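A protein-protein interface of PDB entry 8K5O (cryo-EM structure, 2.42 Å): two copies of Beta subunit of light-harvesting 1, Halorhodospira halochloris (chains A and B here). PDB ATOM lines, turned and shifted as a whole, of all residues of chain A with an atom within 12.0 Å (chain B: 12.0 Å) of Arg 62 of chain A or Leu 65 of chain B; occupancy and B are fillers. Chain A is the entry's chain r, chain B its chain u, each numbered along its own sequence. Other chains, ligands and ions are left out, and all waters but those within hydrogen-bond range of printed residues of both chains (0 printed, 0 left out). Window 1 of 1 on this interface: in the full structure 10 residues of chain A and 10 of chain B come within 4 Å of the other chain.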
ATOM      1  N   ARG A  42      11.308  42.768  -1.116  1.00  0.00           N
ATOM      2  CA  ARG A  42      10.368  41.962  -0.353  1.00  0.00           C
ATOM      3  C   ARG A  42       9.276  42.864   0.194  1.00  0.00           C
ATOM      4  O   ARG A  42       9.543  43.679   1.085  1.00  0.00           O
ATOM      5  CB  ARG A  42      11.064  41.213   0.782  1.00  0.00           C
ATOM      6  CG  ARG A  42      11.911  40.074   0.293  1.00  0.00           C
ATOM      7  CD  ARG A  42      12.467  39.239   1.390  1.00  0.00           C
ATOM      8  NE  ARG A  42      13.186  38.108   0.823  1.00  0.00           N
ATOM      9  CZ  ARG A  42      13.710  37.119   1.530  1.00  0.00           C
ATOM     10  NH1 ARG A  42      13.596  37.074   2.845  1.00  0.00           N
ATOM     11  NH2 ARG A  42      14.338  36.137   0.895  1.00  0.00           N
ATOM     12  N   ASN A  51       3.257  35.705   4.944  1.00  0.00           N
ATOM     13  CA  ASN A  51       4.497  35.365   4.262  1.00  0.00           C
ATOM     14  C   ASN A  51       5.450  34.632   5.192  1.00  0.00           C
ATOM     15  O   ASN A  51       6.671  34.722   5.032  1.00  0.00           O
ATOM     16  CB  ASN A  51       5.179  36.601   3.658  1.00  0.00           C
ATOM     17  CG  ASN A  51       5.280  37.758   4.624  1.00  0.00           C
ATOM     18  OD1 ASN A  51       5.614  37.587   5.791  1.00  0.00           O
ATOM     19  ND2 ASN A  51       5.010  38.954   4.129  1.00  0.00           N
ATOM     20  N   ARG A  52       4.911  33.907   6.166  1.00  0.00           N
ATOM     21  CA  ARG A  52       5.723  33.000   6.959  1.00  0.00           C
ATOM     22  C   ARG A  52       6.182  31.839   6.089  1.00  0.00           C
ATOM     23  O   ARG A  52       5.410  31.297   5.296  1.00  0.00           O
ATOM     24  CB  ARG A  52       4.929  32.479   8.157  1.00  0.00           C
ATOM     25  CG  ARG A  52       4.420  33.565   9.084  1.00  0.00           C
ATOM     26  CD  ARG A  52       3.813  33.008  10.355  1.00  0.00           C
ATOM     27  NE  ARG A  52       2.681  32.132  10.085  1.00  0.00           N
ATOM     28  CZ  ARG A  52       1.857  31.663  11.012  1.00  0.00           C
ATOM     29  NH1 ARG A  52       2.001  31.978  12.288  1.00  0.00           N
ATOM     30  NH2 ARG A  52       0.865  30.858  10.650  1.00  0.00           N
ATOM     31  N   LEU A  53       7.453  31.466   6.231  1.00  0.00           N
ATOM     32  CA  LEU A  53       7.965  30.322   5.487  1.00  0.00           C
ATOM     33  C   LEU A  53       7.266  29.036   5.897  1.00  0.00           C
ATOM     34  O   LEU A  53       7.087  28.138   5.069  1.00  0.00           O
ATOM     35  CB  LEU A  53       9.472  30.191   5.691  1.00  0.00           C
ATOM     36  CG  LEU A  53      10.364  31.172   4.934  1.00  0.00           C
ATOM     37  CD1 LEU A  53      11.820  30.934   5.287  1.00  0.00           C
ATOM     38  CD2 LEU A  53      10.142  31.054   3.444  1.00  0.00           C
ATOM     39  N   GLU A  54       6.862  28.932   7.163  1.00  0.00           N
ATOM     40  CA  GLU A  54       6.189  27.732   7.643  1.00  0.00           C
ATOM     41  C   GLU A  54       4.833  27.525   6.987  1.00  0.00           C
ATOM     42  O   GLU A  54       4.307  26.407   7.016  1.00  0.00           O
ATOM     43  CB  GLU A  54       6.024  27.804   9.157  1.00  0.00           C
ATOM     44  CG  GLU A  54       5.125  28.931   9.612  1.00  0.00           C
ATOM     45  CD  GLU A  54       5.033  29.029  11.112  1.00  0.00           C
ATOM     46  OE1 GLU A  54       5.705  28.240  11.807  1.00  0.00           O
ATOM     47  OE2 GLU A  54       4.284  29.893  11.603  1.00  0.00           O
ATOM     48  N   ASP A  55       4.249  28.569   6.405  1.00  0.00           N
ATOM     49  CA  ASP A  55       2.950  28.451   5.763  1.00  0.00           C
ATOM     50  C   ASP A  55       3.043  28.176   4.270  1.00  0.00           C
ATOM     51  O   ASP A  55       2.055  27.731   3.676  1.00  0.00           O
ATOM     52  CB  ASP A  55       2.131  29.726   5.976  1.00  0.00           C
ATOM     53  CG  ASP A  55       1.764  29.951   7.425  1.00  0.00           C
ATOM     54  OD1 ASP A  55       1.419  28.973   8.116  1.00  0.00           O
ATOM     55  OD2 ASP A  55       1.815  31.113   7.872  1.00  0.00           O
ATOM     56  N   HIS A  56       4.182  28.436   3.656  1.00  0.00           N
ATOM     57  CA  HIS A  56       4.311  28.314   2.208  1.00  0.00           C
ATOM     58  C   HIS A  56       5.488  27.461   1.770  1.00  0.00           C
ATOM     59  O   HIS A  56       5.380  26.747   0.773  1.00  0.00           O
ATOM     60  CB  HIS A  56       4.420  29.712   1.589  1.00  0.00           C
ATOM     61  CG  HIS A  56       3.319  30.632   2.004  1.00  0.00           C
ATOM     62  ND1 HIS A  56       3.412  31.452   3.106  1.00  0.00           N
ATOM     63  CD2 HIS A  56       2.088  30.841   1.483  1.00  0.00           C
ATOM     64  CE1 HIS A  56       2.292  32.136   3.239  1.00  0.00           C
ATOM     65  NE2 HIS A  56       1.473  31.786   2.265  1.00  0.00           N
ATOM     66  N   ALA A  57       6.608  27.522   2.479  1.00  0.00           N
ATOM     67  CA  ALA A  57       7.751  26.709   2.122  1.00  0.00           C
ATOM     68  C   ALA A  57       7.504  25.257   2.512  1.00  0.00           C
ATOM     69  O   ALA A  57       6.707  24.972   3.410  1.00  0.00           O
ATOM     70  CB  ALA A  57       9.012  27.234   2.802  1.00  0.00           C
ATOM     71  N   PRO A  58       8.166  24.317   1.843  1.00  0.00           N
ATOM     72  CA  PRO A  58       8.091  22.918   2.274  1.00  0.00           C
ATOM     73  C   PRO A  58       8.671  22.753   3.669  1.00  0.00           C
ATOM     74  O   PRO A  58       9.426  23.588   4.169  1.00  0.00           O
ATOM     75  CB  PRO A  58       8.918  22.175   1.223  1.00  0.00           C
ATOM     76  CG  PRO A  58       8.921  23.071   0.040  1.00  0.00           C
ATOM     77  CD  PRO A  58       8.904  24.462   0.579  1.00  0.00           C
ATOM     78  N   ASP A  59       8.297  21.644   4.307  1.00  0.00           N
ATOM     79  CA  ASP A  59       8.649  21.441   5.708  1.00  0.00           C
ATOM     80  C   ASP A  59      10.157  21.367   5.923  1.00  0.00           C
ATOM     81  O   ASP A  59      10.639  21.674   7.018  1.00  0.00           O
ATOM     82  CB  ASP A  59       7.962  20.182   6.240  1.00  0.00           C
ATOM     83  CG  ASP A  59       8.295  18.946   5.428  1.00  0.00           C
ATOM     84  OD1 ASP A  59       8.994  19.071   4.400  1.00  0.00           O
ATOM     85  OD2 ASP A  59       7.853  17.846   5.818  1.00  0.00           O
ATOM     86  N   TYR A  60      10.920  20.967   4.902  1.00  0.00           N
ATOM     87  CA  TYR A  60      12.368  20.898   5.067  1.00  0.00           C
ATOM     88  C   TYR A  60      13.026  22.268   5.014  1.00  0.00           C
ATOM     89  O   TYR A  60      14.165  22.410   5.471  1.00  0.00           O
ATOM     90  CB  TYR A  60      12.990  19.983   4.012  1.00  0.00           C
ATOM     91  CG  TYR A  60      12.598  20.291   2.587  1.00  0.00           C
ATOM     92  CD1 TYR A  60      13.172  21.350   1.898  1.00  0.00           C
ATOM     93  CD2 TYR A  60      11.669  19.504   1.923  1.00  0.00           C
ATOM     94  CE1 TYR A  60      12.819  21.625   0.596  1.00  0.00           C
ATOM     95  CE2 TYR A  60      11.313  19.770   0.621  1.00  0.00           C
ATOM     96  CZ  TYR A  60      11.890  20.831  -0.036  1.00  0.00           C
ATOM     97  OH  TYR A  60      11.531  21.092  -1.334  1.00  0.00           O
ATOM     98  N   VAL A  61      12.350  23.273   4.463  1.00  0.00           N
ATOM     99  CA  VAL A  61      12.868  24.637   4.477  1.00  0.00           C
ATOM    100  C   VAL A  61      12.731  25.167   5.899  1.00  0.00           C
ATOM    101  O   VAL A  61      11.618  25.325   6.406  1.00  0.00           O
ATOM    102  CB  VAL A  61      12.130  25.530   3.475  1.00  0.00           C
ATOM    103  CG1 VAL A  61      12.685  26.943   3.520  1.00  0.00           C
ATOM    104  CG2 VAL A  61      12.228  24.952   2.074  1.00  0.00           C
ATOM    105  N   ARG A  62      13.858  25.439   6.548  1.00  0.00           N
ATOM    106  CA  ARG A  62      13.830  25.808   7.955  1.00  0.00           C
ATOM    107  C   ARG A  62      13.255  27.204   8.146  1.00  0.00           C
ATOM    108  O   ARG A  62      13.607  28.143   7.427  1.00  0.00           O
ATOM    109  CB  ARG A  62      15.230  25.733   8.554  1.00  0.00           C
ATOM    110  CG  ARG A  62      15.250  25.910  10.057  1.00  0.00           C
ATOM    111  CD  ARG A  62      16.663  26.054  10.576  1.00  0.00           C
ATOM    112  NE  ARG A  62      17.424  27.068   9.859  1.00  0.00           N
ATOM    113  CZ  ARG A  62      17.393  28.366  10.126  1.00  0.00           C
ATOM    114  NH1 ARG A  62      16.629  28.855  11.088  1.00  0.00           N
ATOM    115  NH2 ARG A  62      18.154  29.192   9.414  1.00  0.00           N
ATOM    116  N   SER A  63      12.362  27.332   9.123  1.00  0.00           N
ATOM    117  CA  SER A  63      11.838  28.611   9.569  1.00  0.00           C
ATOM    118  C   SER A  63      12.109  28.737  11.057  1.00  0.00           C
ATOM    119  O   SER A  63      11.877  27.790  11.814  1.00  0.00           O
ATOM    120  CB  SER A  63      10.340  28.729   9.287  1.00  0.00           C
ATOM    121  OG  SER A  63       9.830  29.968   9.742  1.00  0.00           O
ATOM    122  N   ALA A  64      12.608  29.894  11.474  1.00  0.00           N
ATOM    123  CA  ALA A  64      12.868  30.147  12.883  1.00  0.00           C
ATOM    124  C   ALA A  64      11.654  30.704  13.609  1.00  0.00           C
ATOM    125  O   ALA A  64      11.784  31.153  14.752  1.00  0.00           O
ATOM    126  CB  ALA A  64      14.052  31.099  13.041  1.00  0.00           C
ATOM    127  N   LEU A  65      10.491  30.697  12.970  1.00  0.00           N
ATOM    128  CA  LEU A  65       9.253  31.144  13.590  1.00  0.00           C
ATOM    129  C   LEU A  65       8.456  29.961  14.121  1.00  0.00           C
ATOM    130  O   LEU A  65       8.283  29.812  15.329  1.00  0.00           O
ATOM    131  CB  LEU A  65       8.416  31.937  12.589  1.00  0.00           C
ATOM    132  CG  LEU A  65       8.696  33.432  12.437  1.00  0.00           C
ATOM    133  CD1 LEU A  65      10.072  33.679  11.858  1.00  0.00           C
ATOM    134  CD2 LEU A  65       7.634  34.045  11.538  1.00  0.00           C
ATOM    135  N   GLN B  46      19.311  38.917  -0.300  1.00  0.00           N
ATOM    136  CA  GLN B  46      18.984  37.632  -0.884  1.00  0.00           C
ATOM    137  C   GLN B  46      17.813  37.760  -1.849  1.00  0.00           C
ATOM    138  O   GLN B  46      16.958  38.640  -1.726  1.00  0.00           O
ATOM    139  CB  GLN B  46      18.658  36.618   0.210  1.00  0.00           C
ATOM    140  CG  GLN B  46      17.394  36.910   0.982  1.00  0.00           C
ATOM    141  CD  GLN B  46      17.614  37.858   2.140  1.00  0.00           C
ATOM    142  OE1 GLN B  46      18.493  38.711   2.098  1.00  0.00           O
ATOM    143  NE2 GLN B  46      16.815  37.709   3.184  1.00  0.00           N
ATOM    144  N   ARG B  48      14.429  35.750  -3.635  1.00  0.00           N
ATOM    145  CA  ARG B  48      13.302  35.075  -3.005  1.00  0.00           C
ATOM    146  C   ARG B  48      13.706  33.702  -2.485  1.00  0.00           C
ATOM    147  O   ARG B  48      13.191  33.254  -1.455  1.00  0.00           O
ATOM    148  CB  ARG B  48      12.138  34.973  -3.987  1.00  0.00           C
ATOM    149  CG  ARG B  48      11.712  36.302  -4.583  1.00  0.00           C
ATOM    150  CD  ARG B  48      10.198  36.416  -4.673  1.00  0.00           C
ATOM    151  NE  ARG B  48       9.754  37.786  -4.905  1.00  0.00           N
ATOM    152  CZ  ARG B  48       9.697  38.731  -3.974  1.00  0.00           C
ATOM    153  NH1 ARG B  48      10.047  38.490  -2.722  1.00  0.00           N
ATOM    154  NH2 ARG B  48       9.276  39.946  -4.310  1.00  0.00           N
ATOM    155  N   ALA B  49      14.647  33.041  -3.161  1.00  0.00           N
ATOM    156  CA  ALA B  49      15.191  31.773  -2.695  1.00  0.00           C
ATOM    157  C   ALA B  49      16.032  31.915  -1.434  1.00  0.00           C
ATOM    158  O   ALA B  49      16.320  30.902  -0.789  1.00  0.00           O
ATOM    159  CB  ALA B  49      16.038  31.132  -3.791  1.00  0.00           C
ATOM    160  N   GLY B  50      16.432  33.127  -1.075  1.00  0.00           N
ATOM    161  CA  GLY B  50      17.342  33.324   0.030  1.00  0.00           C
ATOM    162  C   GLY B  50      18.770  33.029  -0.373  1.00  0.00           C
ATOM    163  O   GLY B  50      19.074  32.660  -1.507  1.00  0.00           O
ATOM    164  N   ASN B  51      19.673  33.206   0.587  1.00  0.00           N
ATOM    165  CA  ASN B  51      21.065  32.815   0.406  1.00  0.00           C
ATOM    166  C   ASN B  51      21.574  32.040   1.615  1.00  0.00           C
ATOM    167  O   ASN B  51      22.771  32.040   1.904  1.00  0.00           O
ATOM    168  CB  ASN B  51      21.953  34.028   0.121  1.00  0.00           C
ATOM    169  CG  ASN B  51      21.763  35.142   1.121  1.00  0.00           C
ATOM    170  OD1 ASN B  51      21.612  34.904   2.313  1.00  0.00           O
ATOM    171  ND2 ASN B  51      21.781  36.374   0.637  1.00  0.00           N
ATOM    172  N   ARG B  52      20.673  31.381   2.334  1.00  0.00           N
ATOM    173  CA  ARG B  52      21.082  30.509   3.422  1.00  0.00           C
ATOM    174  C   ARG B  52      21.775  29.274   2.865  1.00  0.00           C
ATOM    175  O   ARG B  52      21.328  28.684   1.879  1.00  0.00           O
ATOM    176  CB  ARG B  52      19.872  30.101   4.261  1.00  0.00           C
ATOM    177  CG  ARG B  52      19.276  31.225   5.073  1.00  0.00           C
ATOM    178  CD  ARG B  52      18.211  30.730   6.030  1.00  0.00           C
ATOM    179  NE  ARG B  52      17.241  29.850   5.395  1.00  0.00           N
ATOM    180  CZ  ARG B  52      16.108  29.459   5.960  1.00  0.00           C
ATOM    181  NH1 ARG B  52      15.763  29.868   7.168  1.00  0.00           N
ATOM    182  NH2 ARG B  52      15.303  28.638   5.296  1.00  0.00           N
ATOM    183  N   LEU B  53      22.880  28.885   3.502  1.00  0.00           N
ATOM    184  CA  LEU B  53      23.613  27.712   3.040  1.00  0.00           C
ATOM    185  C   LEU B  53      22.807  26.437   3.229  1.00  0.00           C
ATOM    186  O   LEU B  53      22.949  25.495   2.443  1.00  0.00           O
ATOM    187  CB  LEU B  53      24.951  27.607   3.767  1.00  0.00           C
ATOM    188  CG  LEU B  53      26.086  28.492   3.255  1.00  0.00           C
ATOM    189  CD1 LEU B  53      27.271  28.403   4.197  1.00  0.00           C
ATOM    190  CD2 LEU B  53      26.485  28.099   1.848  1.00  0.00           C
ATOM    191  N   GLU B  54      21.953  26.387   4.253  1.00  0.00           N
ATOM    192  CA  GLU B  54      21.133  25.202   4.476  1.00  0.00           C
ATOM    193  C   GLU B  54      20.188  24.942   3.313  1.00  0.00           C
ATOM    194  O   GLU B  54      19.861  23.785   3.026  1.00  0.00           O
ATOM    195  CB  GLU B  54      20.335  25.355   5.767  1.00  0.00           C
ATOM    196  CG  GLU B  54      19.525  26.633   5.829  1.00  0.00           C
ATOM    197  CD  GLU B  54      19.209  27.046   7.241  1.00  0.00           C
ATOM    198  OE1 GLU B  54      18.303  26.437   7.838  1.00  0.00           O
ATOM    199  OE2 GLU B  54      19.861  27.976   7.758  1.00  0.00           O
ATOM    200  N   ASP B  55      19.737  25.992   2.636  1.00  0.00           N
ATOM    201  CA  ASP B  55      18.793  25.851   1.541  1.00  0.00           C
ATOM    202  C   ASP B  55      19.458  25.598   0.198  1.00  0.00           C
ATOM    203  O   ASP B  55      18.764  25.240  -0.759  1.00  0.00           O
ATOM    204  CB  ASP B  55      17.912  27.097   1.446  1.00  0.00           C
ATOM    205  CG  ASP B  55      17.094  27.325   2.698  1.00  0.00           C
ATOM    206  OD1 ASP B  55      16.175  26.523   2.966  1.00  0.00           O
ATOM    207  OD2 ASP B  55      17.370  28.305   3.414  1.00  0.00           O
ATOM    208  N   HIS B  56      20.762  25.770   0.094  1.00  0.00           N
ATOM    209  CA  HIS B  56      21.410  25.571  -1.197  1.00  0.00           C
ATOM    210  C   HIS B  56      22.611  24.639  -1.140  1.00  0.00           C
ATOM    211  O   HIS B  56      22.824  23.871  -2.080  1.00  0.00           O
ATOM    212  CB  HIS B  56      21.812  26.932  -1.775  1.00  0.00           C
ATOM    213  CG  HIS B  56      20.701  27.936  -1.765  1.00  0.00           C
ATOM    214  ND1 HIS B  56      20.551  28.871  -0.767  1.00  0.00           N
ATOM    215  CD2 HIS B  56      19.668  28.126  -2.617  1.00  0.00           C
ATOM    216  CE1 HIS B  56      19.482  29.607  -1.013  1.00  0.00           C
ATOM    217  NE2 HIS B  56      18.930  29.177  -2.133  1.00  0.00           N
ATOM    218  N   ALA B  57      23.392  24.681  -0.072  1.00  0.00           N
ATOM    219  CA  ALA B  57      24.529  23.790   0.056  1.00  0.00           C
ATOM    220  C   ALA B  57      24.064  22.389   0.436  1.00  0.00           C
ATOM    221  O   ALA B  57      22.986  22.216   1.008  1.00  0.00           O
ATOM    222  CB  ALA B  57      25.505  24.327   1.096  1.00  0.00           C
ATOM    223  N   PRO B  58      24.858  21.363   0.119  1.00  0.00           N
ATOM    224  CA  PRO B  58      24.488  20.000   0.520  1.00  0.00           C
ATOM    225  C   PRO B  58      24.490  19.815   2.029  1.00  0.00           C
ATOM    226  O   PRO B  58      24.864  20.722   2.778  1.00  0.00           O
ATOM    227  CB  PRO B  58      25.558  19.132  -0.152  1.00  0.00           C
ATOM    228  CG  PRO B  58      26.114  19.973  -1.241  1.00  0.00           C
ATOM    229  CD  PRO B  58      26.052  21.374  -0.742  1.00  0.00           C
ATOM    230  N   ASP B  59      24.074  18.632   2.483  1.00  0.00           N
ATOM    231  CA  ASP B  59      23.942  18.389   3.915  1.00  0.00           C
ATOM    232  C   ASP B  59      25.289  18.453   4.623  1.00  0.00           C
ATOM    233  O   ASP B  59      25.377  18.928   5.760  1.00  0.00           O
ATOM    234  CB  ASP B  59      23.275  17.036   4.154  1.00  0.00           C
ATOM    235  CG  ASP B  59      23.882  15.931   3.314  1.00  0.00           C
ATOM    236  OD1 ASP B  59      23.882  16.058   2.070  1.00  0.00           O
ATOM    237  OD2 ASP B  59      24.364  14.937   3.895  1.00  0.00           O
ATOM    238  N   TYR B  60      26.351  17.972   3.973  1.00  0.00           N
ATOM    239  CA  TYR B  60      27.650  17.917   4.632  1.00  0.00           C
ATOM    240  C   TYR B  60      28.266  19.294   4.831  1.00  0.00           C
ATOM    241  O   TYR B  60      29.159  19.439   5.672  1.00  0.00           O
ATOM    242  CB  TYR B  60      28.613  17.026   3.848  1.00  0.00           C
ATOM    243  CG  TYR B  60      28.693  17.314   2.370  1.00  0.00           C
ATOM    244  CD1 TYR B  60      29.470  18.354   1.885  1.00  0.00           C
ATOM    245  CD2 TYR B  60      28.004  16.531   1.457  1.00  0.00           C
ATOM    246  CE1 TYR B  60      29.553  18.611   0.535  1.00  0.00           C
ATOM    247  CE2 TYR B  60      28.080  16.779   0.107  1.00  0.00           C
ATOM    248  CZ  TYR B  60      28.856  17.821  -0.348  1.00  0.00           C
ATOM    249  OH  TYR B  60      28.930  18.069  -1.696  1.00  0.00           O
ATOM    250  N   VAL B  61      27.819  20.301   4.088  1.00  0.00           N
ATOM    251  CA  VAL B  61      28.302  21.662   4.285  1.00  0.00           C
ATOM    252  C   VAL B  61      27.656  22.202   5.555  1.00  0.00           C
ATOM    253  O   VAL B  61      26.443  22.409   5.606  1.00  0.00           O
ATOM    254  CB  VAL B  61      27.992  22.557   3.082  1.00  0.00           C
ATOM    255  CG1 VAL B  61      28.377  23.995   3.385  1.00  0.00           C
ATOM    256  CG2 VAL B  61      28.718  22.056   1.847  1.00  0.00           C
ATOM    257  N   ARG B  62      28.462  22.412   6.589  1.00  0.00           N
ATOM    258  CA  ARG B  62      27.940  22.951   7.835  1.00  0.00           C
ATOM    259  C   ARG B  62      27.589  24.419   7.665  1.00  0.00           C
ATOM    260  O   ARG B  62      28.285  25.169   6.977  1.00  0.00           O
ATOM    261  CB  ARG B  62      28.951  22.778   8.964  1.00  0.00           C
ATOM    262  CG  ARG B  62      28.344  22.836  10.353  1.00  0.00           C
ATOM    263  CD  ARG B  62      28.584  24.176  11.022  1.00  0.00           C
ATOM    264  NE  ARG B  62      29.971  24.607  10.904  1.00  0.00           N
ATOM    265  CZ  ARG B  62      30.382  25.855  11.076  1.00  0.00           C
ATOM    266  NH1 ARG B  62      29.540  26.825  11.384  1.00  0.00           N
ATOM    267  NH2 ARG B  62      31.673  26.138  10.932  1.00  0.00           N
ATOM    268  N   SER B  63      26.492  24.824   8.286  1.00  0.00           N
ATOM    269  CA  SER B  63      26.067  26.212   8.303  1.00  0.00           C
ATOM    270  C   SER B  63      25.895  26.637   9.751  1.00  0.00           C
ATOM    271  O   SER B  63      25.341  25.886  10.559  1.00  0.00           O
ATOM    272  CB  SER B  63      24.763  26.400   7.523  1.00  0.00           C
ATOM    273  OG  SER B  63      24.290  27.730   7.621  1.00  0.00           O
ATOM    274  N   ALA B  64      26.379  27.831  10.079  1.00  0.00           N
ATOM    275  CA  ALA B  64      26.133  28.419  11.387  1.00  0.00           C
ATOM    276  C   ALA B  64      24.706  28.923  11.530  1.00  0.00           C
ATOM    277  O   ALA B  64      24.408  29.639  12.490  1.00  0.00           O
ATOM    278  CB  ALA B  64      27.122  29.557  11.646  1.00  0.00           C
ATOM    279  N   LEU B  65      23.849  28.576  10.573  1.00  0.00           N
ATOM    280  CA  LEU B  65      22.423  28.880  10.557  1.00  0.00           C
ATOM    281  C   LEU B  65      22.210  30.366  10.292  1.00  0.00           C
ATOM    282  O   LEU B  65      22.467  30.854   9.188  1.00  0.00           O
ATOM    283  CB  LEU B  65      21.744  28.465  11.864  1.00  0.00           C
ATOM    284  CG  LEU B  65      21.336  26.994  12.011  1.00  0.00           C
ATOM    285  CD1 LEU B  65      20.301  26.615  10.991  1.00  0.00           C
ATOM    286  CD2 LEU B  65      22.512  26.034  11.956  1.00  0.00           C
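NH2 of Arg 62 of chain A is in salt-bridge range of OE2 of Glu 54 of chain B (2.7 Å).
The guanidinium group (NH1) of Arg 42 of chain A sits close to the side-chain amide nitrogen (NE2) of Gln 46 of chain B (3.3 Å).
The guanidinium group of Arg 52 of chain B lies within hydrogen-bond range of the backbone carbonyl oxygen of Arg 62 of chain A.
The backbone carbonyl oxygen of Arg 52 of chain B is in hydrogen-bond range of a ring nitrogen (ND1) of His 56 of chain B.
NE of Arg 52 of chain B is in salt-bridge range of OD2 of Asp 55 of chain B.
N of Leu 65 of chain B lies close to OG of Ser 63 of chain B (3.1 Å).
The guanidinium group (NE) of Arg 52 of chain B is in salt-bridge range of the side-chain carboxylate (OE2) of Glu 54 of chain B, at 3.995 Å.
CG of Arg 42 of chain A touches NH1 of Arg 48 of chain B, at 3.9 Å.
NH2 of Arg 52 of chain B touches CG1 of Val 61 of chain A, at 3.6 Å.
Val 61 of chain A touches Asp 55 of chain B (CG1 to OD1, 3.6 Å).
Arg 62 of chain A touches Leu 65 of chain B (NE to CD1, 3.1 Å).
Printed residues of chain B within 4 Å of Arg 42 of chain A: Gln 46 (3.2 Å) and Arg 48 (3.9 Å).
No residue of chain B comes within 4 Å of Leu 53 of chain A.
Of chain B, only Arg 52 and Asp 55 come within 4 Å of Val 61 of chain A.
Of the printed residues of chain B, Arg 62 of chain A touches Arg 52, Glu 54 and Leu 65.
No residue of chain B comes within 4 Å of Ser 63 of chain A.
Printed residues of chain A within 4 Å of Gln 46 of chain B: Arg 42 (3.2 Å).
Of the printed residues of chain A, Arg 48 of chain B touches Arg 42 (3.9 Å).
Arg 52 of chain B touches just these residues of chain A: Val 61 (3.6 Å) and Arg 62 (2.8 Å).
Of the printed residues of chain A, Asp 55 of chain B touches Val 61.
No residue of chain A comes within 4 Å of Ser 63 of chain B.
Of chain A, only Arg 62 (3.1 Å) comes within 4 Å of Leu 65 of chain B.
The nearest residue of chain A that does not touch Leu 65 of chain B is Ala 64 of chain A (8.0 Å).
The nearest printed residue of chain B that does not touch Arg 42 of chain A is Gly 50 of chain B (4.2 Å).
Of the 16 printed residues of chain A, 3 touch a printed residue of chain B.
Hydrophobic or aromatic side chains of chain A within 4 Å of the printed part of chain B: Val 61.
Along chain A the printed residues that touch a printed residue of chain B span positions 42 to 62.
Hydrophobic or aromatic side chains of chain B within 4 Å of the printed part of chain A: Leu 65.
Among the printed residues, Asp or Glu carboxylates within 4 Å of a Lys or Arg side-chain nitrogen of the other chain: Arg 62 of chain A with Glu 54 of chain B (2.3 Å).
Val 61 of chain A touches Asp 55 of chain B, but with the chains exchanged Asp 55 of chain A does not touch Val 61 of chain B (23.0 Å).
Arg 62 of chain A touches Arg 52 of chain B, but with the chains exchanged Arg 52 of chain A does not touch Arg 62 of chain B (22.7 Å).
Arg 62 of chain A touches Glu 54 of chain B, but with the chains exchanged Glu 54 of chain A does not touch Arg 62 of chain B (21.2 Å).
Arg 62 of chain A touches Leu 65 of chain B, but with the chains exchanged Leu 65 of chain A does not touch Arg 62 of chain B (19.0 Å).
Of the 7 pairs that touch across the chains among the printed residues, none has its exchanged pair printed and touching as well.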
